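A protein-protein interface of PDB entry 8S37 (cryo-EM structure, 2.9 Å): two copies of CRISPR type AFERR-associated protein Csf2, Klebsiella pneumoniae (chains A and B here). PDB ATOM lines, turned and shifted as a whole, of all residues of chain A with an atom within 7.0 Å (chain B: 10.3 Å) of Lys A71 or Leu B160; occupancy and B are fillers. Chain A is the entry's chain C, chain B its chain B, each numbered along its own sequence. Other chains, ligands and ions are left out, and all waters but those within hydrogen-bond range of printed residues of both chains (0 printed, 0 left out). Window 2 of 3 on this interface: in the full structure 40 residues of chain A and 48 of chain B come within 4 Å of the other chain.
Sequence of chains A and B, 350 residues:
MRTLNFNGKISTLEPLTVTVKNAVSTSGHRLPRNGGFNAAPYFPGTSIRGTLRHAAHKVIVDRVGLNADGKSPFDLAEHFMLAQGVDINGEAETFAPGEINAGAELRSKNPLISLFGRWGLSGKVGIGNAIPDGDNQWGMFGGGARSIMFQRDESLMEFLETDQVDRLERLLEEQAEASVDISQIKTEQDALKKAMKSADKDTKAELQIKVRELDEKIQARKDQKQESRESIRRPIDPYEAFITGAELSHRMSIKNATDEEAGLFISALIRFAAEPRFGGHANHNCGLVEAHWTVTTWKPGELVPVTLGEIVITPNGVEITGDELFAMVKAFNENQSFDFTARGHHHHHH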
ATOM      1  N   VAL A  61     -21.053 -25.308   7.450  1.00  0.00           N
ATOM      2  CA  VAL A  61     -22.262 -24.861   8.134  1.00  0.00           C
ATOM      3  C   VAL A  61     -23.455 -24.928   7.191  1.00  0.00           C
ATOM      4  O   VAL A  61     -24.534 -25.405   7.562  1.00  0.00           O
ATOM      5  CB  VAL A  61     -22.059 -23.443   8.700  1.00  0.00           C
ATOM      6  CG1 VAL A  61     -23.387 -22.834   9.122  1.00  0.00           C
ATOM      7  CG2 VAL A  61     -21.101 -23.477   9.878  1.00  0.00           C
ATOM      8  N   GLY A  65     -26.580 -27.421   7.273  1.00  0.00           N
ATOM      9  CA  GLY A  65     -27.855 -26.747   7.174  1.00  0.00           C
ATOM     10  C   GLY A  65     -28.301 -26.125   8.485  1.00  0.00           C
ATOM     11  O   GLY A  65     -27.888 -26.517   9.576  1.00  0.00           O
ATOM     12  N   LEU A  66     -29.170 -25.130   8.350  1.00  0.00           N
ATOM     13  CA  LEU A  66     -29.587 -24.261   9.438  1.00  0.00           C
ATOM     14  C   LEU A  66     -31.042 -24.535   9.786  1.00  0.00           C
ATOM     15  O   LEU A  66     -31.875 -24.736   8.896  1.00  0.00           O
ATOM     16  CB  LEU A  66     -29.421 -22.788   9.054  1.00  0.00           C
ATOM     17  CG  LEU A  66     -28.019 -22.174   9.091  1.00  0.00           C
ATOM     18  CD1 LEU A  66     -26.982 -23.045   8.398  1.00  0.00           C
ATOM     19  CD2 LEU A  66     -28.057 -20.798   8.451  1.00  0.00           C
ATOM     20  N   ASN A  67     -31.345 -24.543  11.079  1.00  0.00           N
ATOM     21  CA  ASN A  67     -32.719 -24.730  11.516  1.00  0.00           C
ATOM     22  C   ASN A  67     -33.562 -23.528  11.089  1.00  0.00           C
ATOM     23  O   ASN A  67     -33.060 -22.549  10.528  1.00  0.00           O
ATOM     24  CB  ASN A  67     -32.775 -24.938  13.028  1.00  0.00           C
ATOM     25  CG  ASN A  67     -32.183 -23.776  13.802  1.00  0.00           C
ATOM     26  OD1 ASN A  67     -31.701 -22.805  13.220  1.00  0.00           O
ATOM     27  ND2 ASN A  67     -32.222 -23.871  15.125  1.00  0.00           N
ATOM     28  N   ALA A  68     -34.870 -23.625  11.345  1.00  0.00           N
ATOM     29  CA  ALA A  68     -35.819 -22.627  10.854  1.00  0.00           C
ATOM     30  C   ALA A  68     -35.409 -21.212  11.247  1.00  0.00           C
ATOM     31  O   ALA A  68     -35.412 -20.298  10.415  1.00  0.00           O
ATOM     32  CB  ALA A  68     -37.219 -22.944  11.382  1.00  0.00           C
ATOM     33  N   ASP A  69     -35.048 -21.013  12.516  1.00  0.00           N
ATOM     34  CA  ASP A  69     -34.607 -19.695  12.960  1.00  0.00           C
ATOM     35  C   ASP A  69     -33.303 -19.260  12.297  1.00  0.00           C
ATOM     36  O   ASP A  69     -32.965 -18.072  12.351  1.00  0.00           O
ATOM     37  CB  ASP A  69     -34.442 -19.691  14.480  1.00  0.00           C
ATOM     38  CG  ASP A  69     -34.276 -18.295  15.052  1.00  0.00           C
ATOM     39  OD1 ASP A  69     -34.534 -17.311  14.325  1.00  0.00           O
ATOM     40  OD2 ASP A  69     -33.886 -18.180  16.232  1.00  0.00           O
ATOM     41  N   GLY A  70     -32.570 -20.181  11.679  1.00  0.00           N
ATOM     42  CA  GLY A  70     -31.326 -19.867  11.009  1.00  0.00           C
ATOM     43  C   GLY A  70     -30.078 -20.203  11.794  1.00  0.00           C
ATOM     44  O   GLY A  70     -28.987 -19.785  11.392  1.00  0.00           O
ATOM     45  N   LYS A  71     -30.204 -20.936  12.892  1.00  0.00           N
ATOM     46  CA  LYS A  71     -29.072 -21.293  13.732  1.00  0.00           C
ATOM     47  C   LYS A  71     -28.446 -22.598  13.261  1.00  0.00           C
ATOM     48  O   LYS A  71     -29.109 -23.447  12.658  1.00  0.00           O
ATOM     49  CB  LYS A  71     -29.504 -21.416  15.193  1.00  0.00           C
ATOM     50  CG  LYS A  71     -30.330 -20.239  15.700  1.00  0.00           C
ATOM     51  CD  LYS A  71     -29.656 -18.905  15.416  1.00  0.00           C
ATOM     52  CE  LYS A  71     -30.312 -17.773  16.187  1.00  0.00           C
ATOM     53  NZ  LYS A  71     -29.655 -16.462  15.926  1.00  0.00           N
ATOM     54  N   SER A  72     -27.156 -22.748  13.544  1.00  0.00           N
ATOM     55  CA  SER A  72     -26.406 -23.930  13.148  1.00  0.00           C
ATOM     56  C   SER A  72     -26.336 -24.924  14.303  1.00  0.00           C
ATOM     57  O   SER A  72     -26.233 -24.513  15.464  1.00  0.00           O
ATOM     58  CB  SER A  72     -24.987 -23.555  12.726  1.00  0.00           C
ATOM     59  OG  SER A  72     -24.196 -24.714  12.531  1.00  0.00           O
ATOM     60  N   PRO A  73     -26.398 -26.237  14.053  1.00  0.00           N
ATOM     61  CA  PRO A  73     -26.318 -27.188  15.175  1.00  0.00           C
ATOM     62  C   PRO A  73     -25.023 -27.101  15.960  1.00  0.00           C
ATOM     63  O   PRO A  73     -25.017 -27.418  17.156  1.00  0.00           O
ATOM     64  CB  PRO A  73     -26.462 -28.554  14.490  1.00  0.00           C
ATOM     65  CG  PRO A  73     -27.133 -28.277  13.209  1.00  0.00           C
ATOM     66  CD  PRO A  73     -26.656 -26.931  12.777  1.00  0.00           C
ATOM     67  N   PHE A  74     -23.925 -26.699  15.322  1.00  0.00           N
ATOM     68  CA  PHE A  74     -22.619 -26.747  15.968  1.00  0.00           C
ATOM     69  C   PHE A  74     -22.596 -25.907  17.239  1.00  0.00           C
ATOM     70  O   PHE A  74     -23.141 -24.801  17.287  1.00  0.00           O
ATOM     71  CB  PHE A  74     -21.538 -26.238  15.011  1.00  0.00           C
ATOM     72  CG  PHE A  74     -21.451 -26.988  13.712  1.00  0.00           C
ATOM     73  CD1 PHE A  74     -21.836 -28.315  13.615  1.00  0.00           C
ATOM     74  CD2 PHE A  74     -20.972 -26.353  12.581  1.00  0.00           C
ATOM     75  CE1 PHE A  74     -21.748 -28.985  12.417  1.00  0.00           C
ATOM     76  CE2 PHE A  74     -20.882 -27.020  11.383  1.00  0.00           C
ATOM     77  CZ  PHE A  74     -21.268 -28.337  11.299  1.00  0.00           C
ATOM     78  N   ASP A  75     -21.958 -26.447  18.272  1.00  0.00           N
ATOM     79  CA  ASP A  75     -21.661 -25.683  19.471  1.00  0.00           C
ATOM     80  C   ASP A  75     -20.636 -24.594  19.167  1.00  0.00           C
ATOM     81  O   ASP A  75     -19.898 -24.655  18.180  1.00  0.00           O
ATOM     82  CB  ASP A  75     -21.139 -26.598  20.577  1.00  0.00           C
ATOM     83  CG  ASP A  75     -22.058 -27.772  20.842  1.00  0.00           C
ATOM     84  OD1 ASP A  75     -23.264 -27.662  20.542  1.00  0.00           O
ATOM     85  OD2 ASP A  75     -21.574 -28.806  21.350  1.00  0.00           O
ATOM     86  N   LEU A  76     -20.604 -23.581  20.034  1.00  0.00           N
ATOM     87  CA  LEU A  76     -19.587 -22.539  19.924  1.00  0.00           C
ATOM     88  C   LEU A  76     -18.188 -23.145  19.922  1.00  0.00           C
ATOM     89  O   LEU A  76     -17.318 -22.729  19.144  1.00  0.00           O
ATOM     90  CB  LEU A  76     -19.738 -21.551  21.080  1.00  0.00           C
ATOM     91  CG  LEU A  76     -18.928 -20.260  20.993  1.00  0.00           C
ATOM     92  CD1 LEU A  76     -19.663 -19.223  20.167  1.00  0.00           C
ATOM     93  CD2 LEU A  76     -18.620 -19.726  22.382  1.00  0.00           C
ATOM     94  N   HIS A  79     -17.686 -24.491  16.497  1.00  0.00           N
ATOM     95  CA  HIS A  79     -17.354 -23.432  15.549  1.00  0.00           C
ATOM     96  C   HIS A  79     -15.886 -23.045  15.660  1.00  0.00           C
ATOM     97  O   HIS A  79     -15.176 -22.949  14.649  1.00  0.00           O
ATOM     98  CB  HIS A  79     -18.229 -22.202  15.806  1.00  0.00           C
ATOM     99  CG  HIS A  79     -19.606 -22.292  15.229  1.00  0.00           C
ATOM    100  ND1 HIS A  79     -19.962 -21.668  14.053  1.00  0.00           N
ATOM    101  CD2 HIS A  79     -20.726 -22.904  15.681  1.00  0.00           C
ATOM    102  CE1 HIS A  79     -21.234 -21.909  13.794  1.00  0.00           C
ATOM    103  NE2 HIS A  79     -21.722 -22.657  14.767  1.00  0.00           N
ATOM    104  N   ILE B 148     -10.956 -13.565  17.172  1.00  0.00           N
ATOM    105  CA  ILE B 148     -12.299 -14.067  17.435  1.00  0.00           C
ATOM    106  C   ILE B 148     -13.087 -14.022  16.137  1.00  0.00           C
ATOM    107  O   ILE B 148     -13.270 -12.953  15.542  1.00  0.00           O
ATOM    108  CB  ILE B 148     -12.988 -13.246  18.530  1.00  0.00           C
ATOM    109  CG1 ILE B 148     -12.238 -13.351  19.863  1.00  0.00           C
ATOM    110  CG2 ILE B 148     -14.437 -13.694  18.691  1.00  0.00           C
ATOM    111  CD1 ILE B 148     -12.360 -14.681  20.569  1.00  0.00           C
ATOM    112  N   MET B 149     -13.535 -15.194  15.681  1.00  0.00           N
ATOM    113  CA  MET B 149     -14.301 -15.283  14.441  1.00  0.00           C
ATOM    114  C   MET B 149     -15.475 -14.311  14.419  1.00  0.00           C
ATOM    115  O   MET B 149     -15.730 -13.656  13.403  1.00  0.00           O
ATOM    116  CB  MET B 149     -14.793 -16.716  14.238  1.00  0.00           C
ATOM    117  CG  MET B 149     -15.432 -17.348  15.466  1.00  0.00           C
ATOM    118  SD  MET B 149     -16.452 -18.770  15.065  1.00  0.00           S
ATOM    119  CE  MET B 149     -15.243 -19.854  14.356  1.00  0.00           C
ATOM    120  N   PHE B 150     -16.201 -14.199  15.531  1.00  0.00           N
ATOM    121  CA  PHE B 150     -17.441 -13.436  15.531  1.00  0.00           C
ATOM    122  C   PHE B 150     -17.220 -11.937  15.660  1.00  0.00           C
ATOM    123  O   PHE B 150     -18.121 -11.164  15.318  1.00  0.00           O
ATOM    124  CB  PHE B 150     -18.344 -13.911  16.667  1.00  0.00           C
ATOM    125  CG  PHE B 150     -18.680 -15.368  16.600  1.00  0.00           C
ATOM    126  CD1 PHE B 150     -19.468 -15.862  15.578  1.00  0.00           C
ATOM    127  CD2 PHE B 150     -18.216 -16.244  17.562  1.00  0.00           C
ATOM    128  CE1 PHE B 150     -19.780 -17.203  15.514  1.00  0.00           C
ATOM    129  CE2 PHE B 150     -18.527 -17.583  17.503  1.00  0.00           C
ATOM    130  CZ  PHE B 150     -19.314 -18.062  16.481  1.00  0.00           C
ATOM    131  N   GLN B 151     -16.055 -11.507  16.135  1.00  0.00           N
ATOM    132  CA  GLN B 151     -15.744 -10.088  16.209  1.00  0.00           C
ATOM    133  C   GLN B 151     -15.136  -9.551  14.923  1.00  0.00           C
ATOM    134  O   GLN B 151     -14.954  -8.335  14.807  1.00  0.00           O
ATOM    135  CB  GLN B 151     -14.791  -9.816  17.375  1.00  0.00           C
ATOM    136  CG  GLN B 151     -15.433  -9.979  18.740  1.00  0.00           C
ATOM    137  CD  GLN B 151     -14.443  -9.790  19.870  1.00  0.00           C
ATOM    138  OE1 GLN B 151     -13.237  -9.717  19.645  1.00  0.00           O
ATOM    139  NE2 GLN B 151     -14.949  -9.710  21.094  1.00  0.00           N
ATOM    140  N   ASP B 153     -16.358 -10.909  11.609  1.00  0.00           N
ATOM    141  CA  ASP B 153     -17.569 -10.898  10.801  1.00  0.00           C
ATOM    142  C   ASP B 153     -18.750 -11.213  11.705  1.00  0.00           C
ATOM    143  O   ASP B 153     -18.725 -12.210  12.434  1.00  0.00           O
ATOM    144  CB  ASP B 153     -17.479 -11.901   9.649  1.00  0.00           C
ATOM    145  CG  ASP B 153     -17.327 -13.325  10.127  1.00  0.00           C
ATOM    146  OD1 ASP B 153     -18.353 -13.939  10.480  1.00  0.00           O
ATOM    147  OD2 ASP B 153     -16.185 -13.829  10.154  1.00  0.00           O
ATOM    148  N   GLU B 154     -19.770 -10.361  11.677  1.00  0.00           N
ATOM    149  CA  GLU B 154     -20.977 -10.649  12.439  1.00  0.00           C
ATOM    150  C   GLU B 154     -21.879 -11.659  11.744  1.00  0.00           C
ATOM    151  O   GLU B 154     -22.813 -12.166  12.374  1.00  0.00           O
ATOM    152  CB  GLU B 154     -21.767  -9.361  12.693  1.00  0.00           C
ATOM    153  CG  GLU B 154     -21.078  -8.357  13.611  1.00  0.00           C
ATOM    154  CD  GLU B 154     -19.956  -7.597  12.929  1.00  0.00           C
ATOM    155  OE1 GLU B 154     -19.595  -7.965  11.791  1.00  0.00           O
ATOM    156  OE2 GLU B 154     -19.437  -6.634  13.530  1.00  0.00           O
ATOM    157  N   SER B 155     -21.615 -11.980  10.474  1.00  0.00           N
ATOM    158  CA  SER B 155     -22.489 -12.901   9.759  1.00  0.00           C
ATOM    159  C   SER B 155     -22.381 -14.319  10.297  1.00  0.00           C
ATOM    160  O   SER B 155     -23.330 -15.100  10.169  1.00  0.00           O
ATOM    161  CB  SER B 155     -22.159 -12.879   8.269  1.00  0.00           C
ATOM    162  OG  SER B 155     -20.806 -13.234   8.044  1.00  0.00           O
ATOM    163  N   LEU B 156     -21.247 -14.675  10.905  1.00  0.00           N
ATOM    164  CA  LEU B 156     -21.150 -15.969  11.566  1.00  0.00           C
ATOM    165  C   LEU B 156     -21.933 -16.019  12.870  1.00  0.00           C
ATOM    166  O   LEU B 156     -22.072 -17.105  13.443  1.00  0.00           O
ATOM    167  CB  LEU B 156     -19.686 -16.318  11.841  1.00  0.00           C
ATOM    168  CG  LEU B 156     -18.865 -16.833  10.655  1.00  0.00           C
ATOM    169  CD1 LEU B 156     -17.380 -16.838  10.986  1.00  0.00           C
ATOM    170  CD2 LEU B 156     -19.317 -18.226  10.249  1.00  0.00           C
ATOM    171  N   MET B 157     -22.467 -14.890  13.333  1.00  0.00           N
ATOM    172  CA  MET B 157     -23.197 -14.854  14.590  1.00  0.00           C
ATOM    173  C   MET B 157     -24.670 -15.193  14.428  1.00  0.00           C
ATOM    174  O   MET B 157     -25.331 -15.516  15.422  1.00  0.00           O
ATOM    175  CB  MET B 157     -23.061 -13.473  15.232  1.00  0.00           C
ATOM    176  CG  MET B 157     -23.602 -13.412  16.637  1.00  0.00           C
ATOM    177  SD  MET B 157     -22.617 -12.366  17.716  1.00  0.00           S
ATOM    178  CE  MET B 157     -23.101 -13.040  19.296  1.00  0.00           C
ATOM    179  N   GLU B 158     -25.193 -15.138  13.204  1.00  0.00           N
ATOM    180  CA  GLU B 158     -26.567 -15.544  12.944  1.00  0.00           C
ATOM    181  C   GLU B 158     -26.759 -17.049  13.054  1.00  0.00           C
ATOM    182  O   GLU B 158     -27.904 -17.512  13.054  1.00  0.00           O
ATOM    183  CB  GLU B 158     -26.993 -15.065  11.556  1.00  0.00           C
ATOM    184  CG  GLU B 158     -26.852 -13.565  11.365  1.00  0.00           C
ATOM    185  CD  GLU B 158     -27.408 -13.093  10.041  1.00  0.00           C
ATOM    186  OE1 GLU B 158     -27.786 -13.949   9.214  1.00  0.00           O
ATOM    187  OE2 GLU B 158     -27.470 -11.863   9.829  1.00  0.00           O
ATOM    188  N   PHE B 159     -25.676 -17.816  13.149  1.00  0.00           N
ATOM    189  CA  PHE B 159     -25.725 -19.268  13.199  1.00  0.00           C
ATOM    190  C   PHE B 159     -25.715 -19.806  14.627  1.00  0.00           C
ATOM    191  O   PHE B 159     -25.656 -21.026  14.812  1.00  0.00           O
ATOM    192  CB  PHE B 159     -24.546 -19.856  12.417  1.00  0.00           C
ATOM    193  CG  PHE B 159     -24.379 -19.279  11.035  1.00  0.00           C
ATOM    194  CD1 PHE B 159     -25.479 -18.918  10.273  1.00  0.00           C
ATOM    195  CD2 PHE B 159     -23.117 -19.097  10.499  1.00  0.00           C
ATOM    196  CE1 PHE B 159     -25.321 -18.386   9.008  1.00  0.00           C
ATOM    197  CE2 PHE B 159     -22.955 -18.568   9.233  1.00  0.00           C
ATOM    198  CZ  PHE B 159     -24.059 -18.214   8.488  1.00  0.00           C
ATOM    199  N   LEU B 160     -25.777 -18.932  15.630  1.00  0.00           N
ATOM    200  CA  LEU B 160     -25.627 -19.303  17.030  1.00  0.00           C
ATOM    201  C   LEU B 160     -26.922 -19.063  17.791  1.00  0.00           C
ATOM    202  O   LEU B 160     -27.555 -18.014  17.643  1.00  0.00           O
ATOM    203  CB  LEU B 160     -24.520 -18.492  17.699  1.00  0.00           C
ATOM    204  CG  LEU B 160     -23.099 -18.609  17.163  1.00  0.00           C
ATOM    205  CD1 LEU B 160     -22.210 -17.661  17.947  1.00  0.00           C
ATOM    206  CD2 LEU B 160     -22.592 -20.039  17.254  1.00  0.00           C
ATOM    207  N   GLU B 161     -27.302 -20.036  18.613  1.00  0.00           N
ATOM    208  CA  GLU B 161     -28.450 -19.866  19.485  1.00  0.00           C
ATOM    209  C   GLU B 161     -28.122 -18.870  20.595  1.00  0.00           C
ATOM    210  O   GLU B 161     -26.964 -18.505  20.822  1.00  0.00           O
ATOM    211  CB  GLU B 161     -28.876 -21.204  20.091  1.00  0.00           C
ATOM    212  CG  GLU B 161     -29.500 -22.180  19.106  1.00  0.00           C
ATOM    213  CD  GLU B 161     -28.475 -22.868  18.226  1.00  0.00           C
ATOM    214  OE1 GLU B 161     -27.283 -22.499  18.294  1.00  0.00           O
ATOM    215  OE2 GLU B 161     -28.862 -23.780  17.466  1.00  0.00           O
ATOM    216  N   THR B 162     -29.169 -18.429  21.294  1.00  0.00           N
ATOM    217  CA  THR B 162     -28.996 -17.439  22.353  1.00  0.00           C
ATOM    218  C   THR B 162     -28.048 -17.944  23.433  1.00  0.00           C
ATOM    219  O   THR B 162     -27.183 -17.198  23.907  1.00  0.00           O
ATOM    220  CB  THR B 162     -30.352 -17.079  22.959  1.00  0.00           C
ATOM    221  OG1 THR B 162     -31.226 -16.604  21.928  1.00  0.00           O
ATOM    222  CG2 THR B 162     -30.195 -16.002  24.025  1.00  0.00           C
ATOM    223  N   ASP B 163     -28.215 -19.200  23.855  1.00  0.00           N
ATOM    224  CA  ASP B 163     -27.329 -19.757  24.872  1.00  0.00           C
ATOM    225  C   ASP B 163     -25.878 -19.727  24.412  1.00  0.00           C
ATOM    226  O   ASP B 163     -24.980 -19.398  25.194  1.00  0.00           O
ATOM    227  CB  ASP B 163     -27.756 -21.186  25.213  1.00  0.00           C
ATOM    228  CG  ASP B 163     -27.790 -22.091  24.000  1.00  0.00           C
ATOM    229  OD1 ASP B 163     -27.575 -21.588  22.878  1.00  0.00           O
ATOM    230  OD2 ASP B 163     -28.030 -23.306  24.165  1.00  0.00           O
ATOM    231  N   GLN B 164     -25.626 -20.047  23.143  1.00  0.00           N
ATOM    232  CA  GLN B 164     -24.258 -19.992  22.638  1.00  0.00           C
ATOM    233  C   GLN B 164     -23.753 -18.558  22.550  1.00  0.00           C
ATOM    234  O   GLN B 164     -22.559 -18.309  22.745  1.00  0.00           O
ATOM    235  CB  GLN B 164     -24.173 -20.672  21.272  1.00  0.00           C
ATOM    236  CG  GLN B 164     -24.571 -22.140  21.281  1.00  0.00           C
ATOM    237  CD  GLN B 164     -23.665 -22.986  22.153  1.00  0.00           C
ATOM    238  OE1 GLN B 164     -22.537 -22.601  22.453  1.00  0.00           O
ATOM    239  NE2 GLN B 164     -24.161 -24.143  22.571  1.00  0.00           N
ATOM    240  N   VAL B 165     -24.636 -17.604  22.257  1.00  0.00           N
ATOM    241  CA  VAL B 165     -24.214 -16.207  22.240  1.00  0.00           C
ATOM    242  C   VAL B 165     -23.801 -15.762  23.637  1.00  0.00           C
ATOM    243  O   VAL B 165     -22.778 -15.088  23.815  1.00  0.00           O
ATOM    244  CB  VAL B 165     -25.339 -15.326  21.671  1.00  0.00           C
ATOM    245  CG1 VAL B 165     -25.055 -13.855  21.924  1.00  0.00           C
ATOM    246  CG2 VAL B 165     -25.511 -15.589  20.182  1.00  0.00           C
ATOM    247  N   ASP B 166     -24.578 -16.137  24.654  1.00  0.00           N
ATOM    248  CA  ASP B 166     -24.178 -15.810  26.016  1.00  0.00           C
ATOM    249  C   ASP B 166     -22.925 -16.571  26.422  1.00  0.00           C
ATOM    250  O   ASP B 166     -22.128 -16.071  27.221  1.00  0.00           O
ATOM    251  CB  ASP B 166     -25.317 -16.116  26.987  1.00  0.00           C
ATOM    252  CG  ASP B 166     -26.584 -15.355  26.654  1.00  0.00           C
ATOM    253  OD1 ASP B 166     -26.481 -14.251  26.080  1.00  0.00           O
ATOM    254  OD2 ASP B 166     -27.682 -15.861  26.967  1.00  0.00           O
ATOM    255  N   ARG B 167     -22.722 -17.764  25.862  1.00  0.00           N
ATOM    256  CA  ARG B 167     -21.480 -18.487  26.102  1.00  0.00           C
ATOM    257  C   ARG B 167     -20.292 -17.713  25.553  1.00  0.00           C
ATOM    258  O   ARG B 167     -19.247 -17.619  26.202  1.00  0.00           O
ATOM    259  CB  ARG B 167     -21.563 -19.878  25.471  1.00  0.00           C
ATOM    260  CG  ARG B 167     -20.356 -20.766  25.711  1.00  0.00           C
ATOM    261  CD  ARG B 167     -20.571 -22.137  25.091  1.00  0.00           C
ATOM    262  NE  ARG B 167     -19.425 -23.021  25.273  1.00  0.00           N
ATOM    263  CZ  ARG B 167     -19.361 -24.272  24.838  1.00  0.00           C
ATOM    264  NH1 ARG B 167     -20.365 -24.832  24.181  1.00  0.00           N
ATOM    265  NH2 ARG B 167     -18.262 -24.983  25.070  1.00  0.00           N
ATOM    266  N   LEU B 168     -20.432 -17.159  24.348  1.00  0.00           N
ATOM    267  CA  LEU B 168     -19.369 -16.328  23.793  1.00  0.00           C
ATOM    268  C   LEU B 168     -19.145 -15.081  24.639  1.00  0.00           C
ATOM    269  O   LEU B 168     -18.002 -14.651  24.835  1.00  0.00           O
ATOM    270  CB  LEU B 168     -19.708 -15.941  22.354  1.00  0.00           C
ATOM    271  CG  LEU B 168     -18.672 -15.109  21.594  1.00  0.00           C
ATOM    272  CD1 LEU B 168     -17.410 -15.915  21.338  1.00  0.00           C
ATOM    273  CD2 LEU B 168     -19.262 -14.603  20.292  1.00  0.00           C
ATOM    274  N   GLU B 169     -20.227 -14.474  25.131  1.00  0.00           N
ATOM    275  CA  GLU B 169     -20.094 -13.330  26.030  1.00  0.00           C
ATOM    276  C   GLU B 169     -19.271 -13.694  27.260  1.00  0.00           C
ATOM    277  O   GLU B 169     -18.346 -12.968  27.648  1.00  0.00           O
ATOM    278  CB  GLU B 169     -21.476 -12.821  26.441  1.00  0.00           C
ATOM    279  CG  GLU B 169     -22.211 -12.055  25.351  1.00  0.00           C
ATOM    280  CD  GLU B 169     -21.646 -10.664  25.126  1.00  0.00           C
ATOM    281  OE1 GLU B 169     -20.577 -10.350  25.691  1.00  0.00           O
ATOM    282  OE2 GLU B 169     -22.276  -9.879  24.387  1.00  0.00           O
ATOM    283  N   LEU B 171     -17.187 -16.161  27.543  1.00  0.00           N
ATOM    284  CA  LEU B 171     -15.825 -16.464  27.126  1.00  0.00           C
ATOM    285  C   LEU B 171     -15.007 -15.192  26.985  1.00  0.00           C
ATOM    286  O   LEU B 171     -13.861 -15.127  27.438  1.00  0.00           O
ATOM    287  CB  LEU B 171     -15.848 -17.224  25.800  1.00  0.00           C
ATOM    288  CG  LEU B 171     -14.622 -18.077  25.465  1.00  0.00           C
ATOM    289  CD1 LEU B 171     -14.972 -19.081  24.381  1.00  0.00           C
ATOM    290  CD2 LEU B 171     -13.438 -17.224  25.032  1.00  0.00           C
ATOM    291  N   LEU B 172     -15.593 -14.158  26.385  1.00  0.00           N
ATOM    292  CA  LEU B 172     -14.850 -12.925  26.162  1.00  0.00           C
ATOM    293  C   LEU B 172     -14.606 -12.182  27.469  1.00  0.00           C
ATOM    294  O   LEU B 172     -13.512 -11.648  27.687  1.00  0.00           O
ATOM    295  CB  LEU B 172     -15.595 -12.047  25.161  1.00  0.00           C
ATOM    296  CG  LEU B 172     -15.688 -12.659  23.762  1.00  0.00           C
ATOM    297  CD1 LEU B 172     -16.725 -11.932  22.943  1.00  0.00           C
ATOM    298  CD2 LEU B 172     -14.340 -12.625  23.059  1.00  0.00           C
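The side-chain carboxylate (OE2) of Glu B161 lies close to the backbone carbonyl oxygen (O) of Ser A72, 3.4 Å away. O of Gly A70 sits close to O of Glu B158, 3.0 Å away. The backbone carbonyl oxygen (O) of Leu B160 lies within hydrogen-bond range of the side-chain amino group (NZ) of Lys A71, 3.1 Å away. The backbone carbonyl oxygen (O) of Phe B159 is in hydrogen-bond range of the backbone NH (N) of Ser A72, 2.6 Å away. OE1 of Gln B164 lies within hydrogen-bond range of N of Leu A76, at 3.2 Å.
OG of Ser A72 lies close to N of Phe A74, at 3.4 Å. OD1 of Asn A67 is in hydrogen-bond range of N of Gly A70, at 3.2 Å. N of Lys A71 sits at hydrogen-bond distance from OD1 of Asn A67 (2.4 Å).
Among the printed residues, pairs that only touch across the chains: His A79 with Met B149, Lys A71 with Glu B158, Leu A76 with Phe B150, Lys A71 with Glu B161, Lys A71 with Phe B159, Leu A66 with Phe B159, Leu A76 with Leu B168, His A79 with Leu B160, Leu A76 with Leu B160, Gly A70 with Phe B159, Leu A76 with Arg B167 and Val A61 with Phe B159.
Leu A66 touches just one residue of chain B: Phe B159 (3.7 Å). No residue of chain B comes within 4 Å of Asn A67. No residue of chain B comes within 4 Å of Asp A69. Of chain B, only Glu B158, Phe B159, Leu B160 and Glu B161 come within 4 Å of Lys A71. Of chain B, only Phe B159 and Glu B161 come within 4 Å of Ser A72. Leu A76 touches five residues of chain B. Of the printed residues of chain A, Phe B150 touches Leu A76 (3.3 Å). Leu B156 touches none of the printed residues of chain A. Of the printed residues of chain A, Phe B159 touches Val A61, Leu A66, Gly A70, Lys A71 and Ser A72. Leu B160 touches just these residues of chain A: Lys A71 (3.1 Å), Leu A76 (3.7 Å) and His A79 (3.7 Å). Printed residues of chain A within 4 Å of Gln B164: Leu A76. Printed residues of chain A within 4 Å of Arg B167: Leu A76. Printed residues of chain A within 4 Å of Leu B168: Leu A76 (3.7 Å). The nearest residue of chain B that does not touch Lys A71 is Met B157 (4.5 Å). The nearest residue of chain A that does not touch Leu B160 is Ser A72 (4.6 Å).
Of the 14 printed residues of chain A, 7 touch a printed residue of chain B. Printed residues of chain A that touch a printed residue of chain B: Val A61, Leu A66, Gly A70, Lys A71, Ser A72, Leu A76 and His A79. Of the 23 printed residues of chain B, 9 touch a printed residue of chain A. Hydrophobic or aromatic side chains of chain B within 4 Å of the printed part of chain A: Met B149, Phe B150, Phe B159, Leu B160 and Leu B168. Among the printed residues, no Asp or Glu carboxylate lies within 4 Å of a Lys or Arg side-chain nitrogen of the other chain.
No position is printed for both chains. Of the 17 pairs that touch across the chains among the printed residues, none has its exchanged pair printed and touching as well.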
